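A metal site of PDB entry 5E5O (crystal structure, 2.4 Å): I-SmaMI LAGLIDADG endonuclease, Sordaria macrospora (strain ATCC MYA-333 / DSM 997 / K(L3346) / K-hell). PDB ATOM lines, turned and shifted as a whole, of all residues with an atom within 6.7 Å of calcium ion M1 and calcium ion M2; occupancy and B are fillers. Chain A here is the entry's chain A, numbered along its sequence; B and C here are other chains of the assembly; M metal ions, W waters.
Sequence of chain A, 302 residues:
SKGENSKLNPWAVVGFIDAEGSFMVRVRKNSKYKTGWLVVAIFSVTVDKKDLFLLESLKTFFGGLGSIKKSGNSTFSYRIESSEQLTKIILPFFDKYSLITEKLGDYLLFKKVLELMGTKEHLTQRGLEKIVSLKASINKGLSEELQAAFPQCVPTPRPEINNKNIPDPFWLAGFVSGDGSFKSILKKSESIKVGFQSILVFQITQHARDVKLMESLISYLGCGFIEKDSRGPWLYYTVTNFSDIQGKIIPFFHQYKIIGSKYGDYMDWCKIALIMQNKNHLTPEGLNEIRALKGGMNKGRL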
ATOM      1  N   ASP A  18       3.355 -24.995 -16.905  1.00  0.00           N
ATOM      2  CA  ASP A  18       2.518 -24.407 -17.932  1.00  0.00           C
ATOM      3  C   ASP A  18       1.072 -24.834 -17.773  1.00  0.00           C
ATOM      4  O   ASP A  18       0.161 -24.010 -17.900  1.00  0.00           O
ATOM      5  CB  ASP A  18       3.018 -24.752 -19.363  1.00  0.00           C
ATOM      6  CG  ASP A  18       3.747 -23.610 -20.020  1.00  0.00           C
ATOM      7  OD1 ASP A  18       3.281 -22.449 -19.904  1.00  0.00           O
ATOM      8  OD2 ASP A  18       4.720 -23.871 -20.732  1.00  0.00           O
ATOM      9  N   ALA A  19       0.854 -26.098 -17.432  1.00  0.00           N
ATOM     10  CA  ALA A  19      -0.468 -26.654 -17.241  1.00  0.00           C
ATOM     11  C   ALA A  19      -1.028 -26.396 -15.875  1.00  0.00           C
ATOM     12  O   ALA A  19      -2.216 -26.167 -15.807  1.00  0.00           O
ATOM     13  CB  ALA A  19      -0.456 -28.179 -17.510  1.00  0.00           C
ATOM     14  N   GLU A  20      -0.262 -26.571 -14.778  1.00  0.00           N
ATOM     15  CA  GLU A  20      -0.851 -26.537 -13.387  1.00  0.00           C
ATOM     16  C   GLU A  20      -0.347 -25.449 -12.381  1.00  0.00           C
ATOM     17  O   GLU A  20      -1.014 -25.128 -11.383  1.00  0.00           O
ATOM     18  CB  GLU A  20      -0.759 -27.899 -12.658  1.00  0.00           C
ATOM     19  CG  GLU A  20      -1.475 -29.137 -13.187  1.00  0.00           C
ATOM     20  CD  GLU A  20      -2.991 -29.017 -13.276  1.00  0.00           C
ATOM     21  OE1 GLU A  20      -3.705 -29.211 -12.260  1.00  0.00           O
ATOM     22  OE2 GLU A  20      -3.517 -28.774 -14.398  1.00  0.00           O
ATOM     23  N   GLY A  21       0.767 -24.829 -12.577  1.00  0.00           N
ATOM     24  CA  GLY A  21       1.127 -23.721 -11.632  1.00  0.00           C
ATOM     25  C   GLY A  21       0.257 -22.479 -11.556  1.00  0.00           C
ATOM     26  O   GLY A  21      -0.513 -22.178 -12.464  1.00  0.00           O
ATOM     27  N   LYS A 103       0.320 -18.562 -19.434  1.00  0.00           N
ATOM     28  CA  LYS A 103       0.903 -18.517 -18.111  1.00  0.00           C
ATOM     29  C   LYS A 103       2.253 -17.740 -18.147  1.00  0.00           C
ATOM     30  O   LYS A 103       2.680 -17.206 -17.145  1.00  0.00           O
ATOM     31  CB  LYS A 103       1.151 -19.955 -17.665  1.00  0.00           C
ATOM     32  CG  LYS A 103       1.551 -20.215 -16.212  1.00  0.00           C
ATOM     33  CD  LYS A 103       0.369 -20.466 -15.314  1.00  0.00           C
ATOM     34  CE  LYS A 103      -0.420 -21.685 -15.715  1.00  0.00           C
ATOM     35  NZ  LYS A 103      -0.371 -22.853 -14.776  1.00  0.00           N
ATOM     36  N   PHE A 175       3.297 -31.355 -19.766  1.00  0.00           N
ATOM     37  CA  PHE A 175       2.067 -30.603 -19.873  1.00  0.00           C
ATOM     38  C   PHE A 175       0.846 -31.517 -19.819  1.00  0.00           C
ATOM     39  O   PHE A 175      -0.142 -31.188 -19.220  1.00  0.00           O
ATOM     40  CB  PHE A 175       2.114 -29.780 -21.137  1.00  0.00           C
ATOM     41  CG  PHE A 175       0.918 -28.978 -21.370  1.00  0.00           C
ATOM     42  CD1 PHE A 175       0.746 -27.828 -20.684  1.00  0.00           C
ATOM     43  CD2 PHE A 175       0.069 -29.282 -22.407  1.00  0.00           C
ATOM     44  CE1 PHE A 175      -0.338 -27.024 -20.894  1.00  0.00           C
ATOM     45  CE2 PHE A 175      -0.988 -28.471 -22.697  1.00  0.00           C
ATOM     46  CZ  PHE A 175      -1.192 -27.340 -21.896  1.00  0.00           C
ATOM     47  N   SER A 177       0.687 -34.312 -18.363  1.00  0.00           N
ATOM     48  CA  SER A 177       0.543 -34.764 -16.996  1.00  0.00           C
ATOM     49  C   SER A 177      -0.387 -33.886 -16.205  1.00  0.00           C
ATOM     50  O   SER A 177      -1.117 -34.406 -15.401  1.00  0.00           O
ATOM     51  CB  SER A 177       1.909 -34.921 -16.309  1.00  0.00           C
ATOM     52  OG  SER A 177       2.744 -35.762 -17.106  1.00  0.00           O
ATOM     53  N   GLY A 178      -0.394 -32.565 -16.453  1.00  0.00           N
ATOM     54  CA  GLY A 178      -1.276 -31.641 -15.717  1.00  0.00           C
ATOM     55  C   GLY A 178      -2.670 -31.472 -16.300  1.00  0.00           C
ATOM     56  O   GLY A 178      -3.681 -31.571 -15.623  1.00  0.00           O
ATOM     57  N   ASP A 179      -2.700 -31.183 -17.566  1.00  0.00           N
ATOM     58  CA  ASP A 179      -3.916 -31.117 -18.322  1.00  0.00           C
ATOM     59  C   ASP A 179      -3.793 -32.192 -19.370  1.00  0.00           C
ATOM     60  O   ASP A 179      -2.748 -32.342 -19.921  1.00  0.00           O
ATOM     61  CB  ASP A 179      -4.008 -29.770 -18.962  1.00  0.00           C
ATOM     62  CG  ASP A 179      -4.179 -28.681 -17.989  1.00  0.00           C
ATOM     63  OD1 ASP A 179      -4.681 -28.973 -16.917  1.00  0.00           O
ATOM     64  OD2 ASP A 179      -3.878 -27.501 -18.241  1.00  0.00           O
ATOM     65  N   GLY A 180      -4.824 -32.967 -19.638  1.00  0.00           N
ATOM     66  CA  GLY A 180      -4.691 -34.143 -20.542  1.00  0.00           C
ATOM     67  C   GLY A 180      -5.477 -35.290 -19.979  1.00  0.00           C
ATOM     68  O   GLY A 180      -5.363 -35.520 -18.807  1.00  0.00           O
ATOM     69  N   THR A 205      -7.607 -30.330 -22.839  1.00  0.00           N
ATOM     70  CA  THR A 205      -8.410 -29.117 -22.607  1.00  0.00           C
ATOM     71  C   THR A 205      -7.539 -27.924 -22.225  1.00  0.00           C
ATOM     72  O   THR A 205      -6.555 -28.047 -21.469  1.00  0.00           O
ATOM     73  CB  THR A 205      -9.525 -29.386 -21.552  1.00  0.00           C
ATOM     74  OG1 THR A 205     -10.206 -30.620 -21.852  1.00  0.00           O
ATOM     75  CG2 THR A 205     -10.535 -28.247 -21.501  1.00  0.00           C
ATOM     76  N   GLN A 206      -7.872 -26.762 -22.766  1.00  0.00           N
ATOM     77  CA  GLN A 206      -7.219 -25.481 -22.450  1.00  0.00           C
ATOM     78  C   GLN A 206      -8.169 -24.377 -22.733  1.00  0.00           C
ATOM     79  O   GLN A 206      -8.909 -24.463 -23.678  1.00  0.00           O
ATOM     80  CB  GLN A 206      -6.067 -25.119 -23.373  1.00  0.00           C
ATOM     81  CG  GLN A 206      -4.700 -25.566 -22.993  1.00  0.00           C
ATOM     82  CD  GLN A 206      -4.303 -25.429 -21.494  1.00  0.00           C
ATOM     83  OE1 GLN A 206      -4.541 -26.404 -20.703  1.00  0.00           O
ATOM     84  NE2 GLN A 206      -3.655 -24.290 -21.139  1.00  0.00           N
ATOM     85  N   LYS A 262      -1.654 -40.328 -13.023  1.00  0.00           N
ATOM     86  CA  LYS A 262      -2.102 -40.392 -14.436  1.00  0.00           C
ATOM     87  C   LYS A 262      -1.278 -41.339 -15.290  1.00  0.00           C
ATOM     88  O   LYS A 262      -1.813 -41.849 -16.260  1.00  0.00           O
ATOM     89  CB  LYS A 262      -2.091 -39.051 -15.095  1.00  0.00           C
ATOM     90  CG  LYS A 262      -2.836 -39.081 -16.425  1.00  0.00           C
ATOM     91  CD  LYS A 262      -2.973 -37.709 -17.019  1.00  0.00           C
ATOM     92  CE  LYS A 262      -4.060 -36.941 -16.290  1.00  0.00           C
ATOM     93  NZ  LYS A 262      -3.673 -35.526 -16.427  1.00  0.00           N
ATOM     94  P    DA B  14     -12.367 -20.240 -16.389  1.00  0.00           P
ATOM     95  OP1  DA B  14     -12.138 -18.894 -15.746  1.00  0.00           O
ATOM     96  OP2  DA B  14     -12.327 -20.307 -17.832  1.00  0.00           O
ATOM     97  O5'  DA B  14     -11.457 -21.280 -15.613  1.00  0.00           O
ATOM     98  C5'  DA B  14     -10.081 -21.504 -15.818  1.00  0.00           C
ATOM     99  C4'  DA B  14      -9.839 -22.997 -15.730  1.00  0.00           C
ATOM    100  O4'  DA B  14     -10.985 -23.769 -15.236  1.00  0.00           O
ATOM    101  C3'  DA B  14      -9.473 -23.643 -17.066  1.00  0.00           C
ATOM    102  O3'  DA B  14      -8.414 -24.538 -16.715  1.00  0.00           O
ATOM    103  C2'  DA B  14     -10.794 -24.264 -17.517  1.00  0.00           C
ATOM    104  C1'  DA B  14     -11.317 -24.774 -16.200  1.00  0.00           C
ATOM    105  N9   DA B  14     -12.751 -25.027 -16.082  1.00  0.00           N
ATOM    106  C8   DA B  14     -13.793 -24.355 -16.678  1.00  0.00           C
ATOM    107  N7   DA B  14     -14.970 -24.724 -16.236  1.00  0.00           N
ATOM    108  C5   DA B  14     -14.679 -25.713 -15.306  1.00  0.00           C
ATOM    109  C6   DA B  14     -15.509 -26.518 -14.490  1.00  0.00           C
ATOM    110  N6   DA B  14     -16.840 -26.439 -14.483  1.00  0.00           N
ATOM    111  N1   DA B  14     -14.904 -27.381 -13.653  1.00  0.00           N
ATOM    112  C2   DA B  14     -13.570 -27.432 -13.627  1.00  0.00           C
ATOM    113  N3   DA B  14     -12.688 -26.742 -14.352  1.00  0.00           N
ATOM    114  C4   DA B  14     -13.323 -25.891 -15.185  1.00  0.00           C
ATOM    115  P    DT B  15      -7.280 -24.884 -17.723  1.00  0.00           P
ATOM    116  OP1  DT B  15      -6.206 -25.582 -17.021  1.00  0.00           O
ATOM    117  OP2  DT B  15      -6.994 -23.738 -18.619  1.00  0.00           O
ATOM    118  O5'  DT B  15      -7.996 -25.748 -18.857  1.00  0.00           O
ATOM    119  C5'  DT B  15      -8.587 -27.069 -18.871  1.00  0.00           C
ATOM    120  C4'  DT B  15      -8.844 -27.761 -17.562  1.00  0.00           C
ATOM    121  O4'  DT B  15     -10.237 -27.474 -17.267  1.00  0.00           O
ATOM    122  C3'  DT B  15      -8.748 -29.284 -17.683  1.00  0.00           C
ATOM    123  O3'  DT B  15      -8.083 -29.987 -16.678  1.00  0.00           O
ATOM    124  C2'  DT B  15     -10.184 -29.761 -17.666  1.00  0.00           C
ATOM    125  C1'  DT B  15     -10.900 -28.663 -16.913  1.00  0.00           C
ATOM    126  N1   DT B  15     -12.313 -28.501 -17.264  1.00  0.00           N
ATOM    127  C2   DT B  15     -13.220 -29.243 -16.529  1.00  0.00           C
ATOM    128  O2   DT B  15     -12.897 -29.998 -15.636  1.00  0.00           O
ATOM    129  N3   DT B  15     -14.536 -29.038 -16.881  1.00  0.00           N
ATOM    130  C4   DT B  15     -15.008 -28.219 -17.886  1.00  0.00           C
ATOM    131  O4   DT B  15     -16.209 -28.141 -18.090  1.00  0.00           O
ATOM    132  C5   DT B  15     -13.997 -27.503 -18.641  1.00  0.00           C
ATOM    133  C7   DT B  15     -14.423 -26.586 -19.742  1.00  0.00           C
ATOM    134  C6   DT B  15     -12.718 -27.679 -18.291  1.00  0.00           C
ATOM    135  P    DC B  16      -7.574 -31.527 -16.938  1.00  0.00           P
ATOM    136  OP1  DC B  16      -6.514 -31.789 -15.891  1.00  0.00           O
ATOM    137  OP2  DC B  16      -7.337 -31.759 -18.388  1.00  0.00           O
ATOM    138  O5'  DC B  16      -8.826 -32.458 -16.657  1.00  0.00           O
ATOM    139  C5'  DC B  16      -9.124 -32.863 -15.323  1.00  0.00           C
ATOM    140  C4'  DC B  16     -10.271 -33.827 -15.376  1.00  0.00           C
ATOM    141  O4'  DC B  16     -11.391 -33.111 -15.920  1.00  0.00           O
ATOM    142  C3'  DC B  16     -10.003 -35.005 -16.324  1.00  0.00           C
ATOM    143  O3'  DC B  16     -10.182 -36.152 -15.504  1.00  0.00           O
ATOM    144  C2'  DC B  16     -10.962 -34.782 -17.489  1.00  0.00           C
ATOM    145  C1'  DC B  16     -12.060 -33.949 -16.841  1.00  0.00           C
ATOM    146  N1   DC B  16     -12.874 -33.101 -17.698  1.00  0.00           N
ATOM    147  C2   DC B  16     -14.226 -32.963 -17.408  1.00  0.00           C
ATOM    148  O2   DC B  16     -14.703 -33.605 -16.469  1.00  0.00           O
ATOM    149  N3   DC B  16     -15.003 -32.160 -18.174  1.00  0.00           N
ATOM    150  C4   DC B  16     -14.447 -31.471 -19.173  1.00  0.00           C
ATOM    151  N4   DC B  16     -15.255 -30.701 -19.914  1.00  0.00           N
ATOM    152  C5   DC B  16     -13.060 -31.557 -19.476  1.00  0.00           C
ATOM    153  C6   DC B  16     -12.310 -32.361 -18.698  1.00  0.00           C
ATOM    154  P    DA C  13     -12.393 -34.098  -7.065  1.00  0.00           P
ATOM    155  OP1  DA C  13     -12.614 -35.465  -7.535  1.00  0.00           O
ATOM    156  OP2  DA C  13     -12.531 -33.731  -5.645  1.00  0.00           O
ATOM    157  O5'  DA C  13     -10.954 -33.807  -7.710  1.00  0.00           O
ATOM    158  C5'  DA C  13     -10.632 -34.191  -9.099  1.00  0.00           C
ATOM    159  C4'  DA C  13      -9.770 -33.152  -9.795  1.00  0.00           C
ATOM    160  O4'  DA C  13     -10.444 -31.873  -9.881  1.00  0.00           O
ATOM    161  C3'  DA C  13      -8.450 -32.809  -9.113  1.00  0.00           C
ATOM    162  O3'  DA C  13      -7.673 -32.036 -10.061  1.00  0.00           O
ATOM    163  C2'  DA C  13      -8.919 -31.813  -8.075  1.00  0.00           C
ATOM    164  C1'  DA C  13      -9.823 -30.965  -8.977  1.00  0.00           C
ATOM    165  N9   DA C  13     -10.906 -30.292  -8.322  1.00  0.00           N
ATOM    166  C8   DA C  13     -11.603 -30.654  -7.201  1.00  0.00           C
ATOM    167  N7   DA C  13     -12.690 -29.949  -7.001  1.00  0.00           N
ATOM    168  C5   DA C  13     -12.729 -29.091  -8.098  1.00  0.00           C
ATOM    169  C6   DA C  13     -13.639 -28.089  -8.473  1.00  0.00           C
ATOM    170  N6   DA C  13     -14.713 -27.762  -7.753  1.00  0.00           N
ATOM    171  N1   DA C  13     -13.395 -27.438  -9.632  1.00  0.00           N
ATOM    172  C2   DA C  13     -12.304 -27.756 -10.338  1.00  0.00           C
ATOM    173  N3   DA C  13     -11.382 -28.668 -10.087  1.00  0.00           N
ATOM    174  C4   DA C  13     -11.667 -29.329  -8.941  1.00  0.00           C
ATOM    175  P    DA C  14      -6.134 -32.299 -10.215  1.00  0.00           P
ATOM    176  OP1  DA C  14      -5.936 -33.056 -11.474  1.00  0.00           O
ATOM    177  OP2  DA C  14      -5.583 -32.667  -8.877  1.00  0.00           O
ATOM    178  O5'  DA C  14      -5.429 -30.893 -10.500  1.00  0.00           O
ATOM    179  C5'  DA C  14      -5.755 -29.685  -9.846  1.00  0.00           C
ATOM    180  C4'  DA C  14      -6.236 -28.714 -10.894  1.00  0.00           C
ATOM    181  O4'  DA C  14      -7.610 -28.329 -10.547  1.00  0.00           O
ATOM    182  C3'  DA C  14      -5.448 -27.416 -10.891  1.00  0.00           C
ATOM    183  O3'  DA C  14      -5.478 -26.822 -12.207  1.00  0.00           O
ATOM    184  C2'  DA C  14      -6.139 -26.642  -9.788  1.00  0.00           C
ATOM    185  C1'  DA C  14      -7.604 -26.979 -10.062  1.00  0.00           C
ATOM    186  N9   DA C  14      -8.501 -26.908  -8.907  1.00  0.00           N
ATOM    187  C8   DA C  14      -8.422 -27.610  -7.732  1.00  0.00           C
ATOM    188  N7   DA C  14      -9.408 -27.377  -6.915  1.00  0.00           N
ATOM    189  C5   DA C  14     -10.194 -26.461  -7.592  1.00  0.00           C
ATOM    190  C6   DA C  14     -11.383 -25.810  -7.244  1.00  0.00           C
ATOM    191  N6   DA C  14     -12.005 -25.991  -6.084  1.00  0.00           N
ATOM    192  N1   DA C  14     -11.933 -24.970  -8.154  1.00  0.00           N
ATOM    193  C2   DA C  14     -11.315 -24.808  -9.325  1.00  0.00           C
ATOM    194  N3   DA C  14     -10.191 -25.374  -9.771  1.00  0.00           N
ATOM    195  C4   DA C  14      -9.660 -26.177  -8.826  1.00  0.00           C
ATOM    196  P    DT C  15      -4.711 -25.396 -12.477  1.00  0.00           P
ATOM    197  OP1  DT C  15      -4.455 -25.356 -13.921  1.00  0.00           O
ATOM    198  OP2  DT C  15      -3.607 -25.191 -11.482  1.00  0.00           O
ATOM    199  O5'  DT C  15      -5.753 -24.288 -11.997  1.00  0.00           O
ATOM    200  C5'  DT C  15      -6.884 -24.052 -12.853  1.00  0.00           C
ATOM    201  C4'  DT C  15      -7.455 -22.680 -12.650  1.00  0.00           C
ATOM    202  O4'  DT C  15      -8.253 -22.649 -11.434  1.00  0.00           O
ATOM    203  C3'  DT C  15      -6.429 -21.555 -12.505  1.00  0.00           C
ATOM    204  O3'  DT C  15      -7.055 -20.436 -13.149  1.00  0.00           O
ATOM    205  C2'  DT C  15      -6.237 -21.485 -10.998  1.00  0.00           C
ATOM    206  C1'  DT C  15      -7.648 -21.796 -10.480  1.00  0.00           C
ATOM    207  N1   DT C  15      -7.817 -22.435  -9.168  1.00  0.00           N
ATOM    208  C2   DT C  15      -9.004 -22.196  -8.530  1.00  0.00           C
ATOM    209  O2   DT C  15      -9.853 -21.438  -8.972  1.00  0.00           O
ATOM    210  N3   DT C  15      -9.139 -22.808  -7.300  1.00  0.00           N
ATOM    211  C4   DT C  15      -8.221 -23.646  -6.685  1.00  0.00           C
ATOM    212  O4   DT C  15      -8.493 -24.123  -5.581  1.00  0.00           O
ATOM    213  C5   DT C  15      -7.006 -23.895  -7.449  1.00  0.00           C
ATOM    214  C7   DT C  15      -5.949 -24.776  -6.872  1.00  0.00           C
ATOM    215  C6   DT C  15      -6.876 -23.296  -8.643  1.00  0.00           C
HETATM  216 CA    CA M   1      -5.402 -30.124 -14.843  1.00  0.00          CA
HETATM  217 CA    CA M   2      -4.478 -26.507 -15.953  1.00  0.00          CA
HETATM  218  O   HOH W   1      -5.058 -31.787 -13.440  1.00  0.00           O
HETATM  219  O   HOH W   2      -3.902 -24.555 -16.926  1.00  0.00           O
HETATM  220  O   HOH W   3      -6.149 -27.564 -14.207  1.00  0.00           O
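Residues that only touch calcium ion M2: DA 14 of chain C (3.9 Å). Along chain A the residues within 4 Å of calcium ion M2 span positions 19 to 179.
Water W1 lies within hydrogen-bond range of OP1 of DA 14 of chain C (2.5 Å) and the side-chain carboxylate (OE1) of Glu 20 (3.1 Å).
Calcium ion M1 is bound by water W1 (2.2 Å), OP1 of DC 16 of chain B (2.3 Å), the side-chain carboxylate (OE2) of Glu 20 (2.4 Å), the backbone carbonyl oxygen (O) of Gly 178 (2.4 Å), the side-chain carboxylate (OD1) of Asp 179 (2.5 Å) and water W3 (2.7 Å). Calcium ion M1 has six donor atoms within binding distance.
Calcium ion M2 is bound by OP1 of DT 15 of chain B, water W2, the backbone carbonyl oxygen (O) of Ala 19, OP1 of DT 15 of chain C, the side-chain carboxylate (OD2) of Asp 179, water W3 and the side-chain carboxylate (OD1) of Asp 179. Slightly farther from calcium ion M2 lies the side-chain carboxylate (OE2) of Glu 20 (2.9 Å).
OP2 of DT 15 of chain C lies close to O of Glu 20. The side-chain carboxylate (OD2) of Asp 179 sits close to the side-chain amide oxygen (OE1) of Gln 206 (2.8 Å). N of Gly 180 sits at hydrogen-bond distance from OP2 of DC 16 of chain B (3.1 Å).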
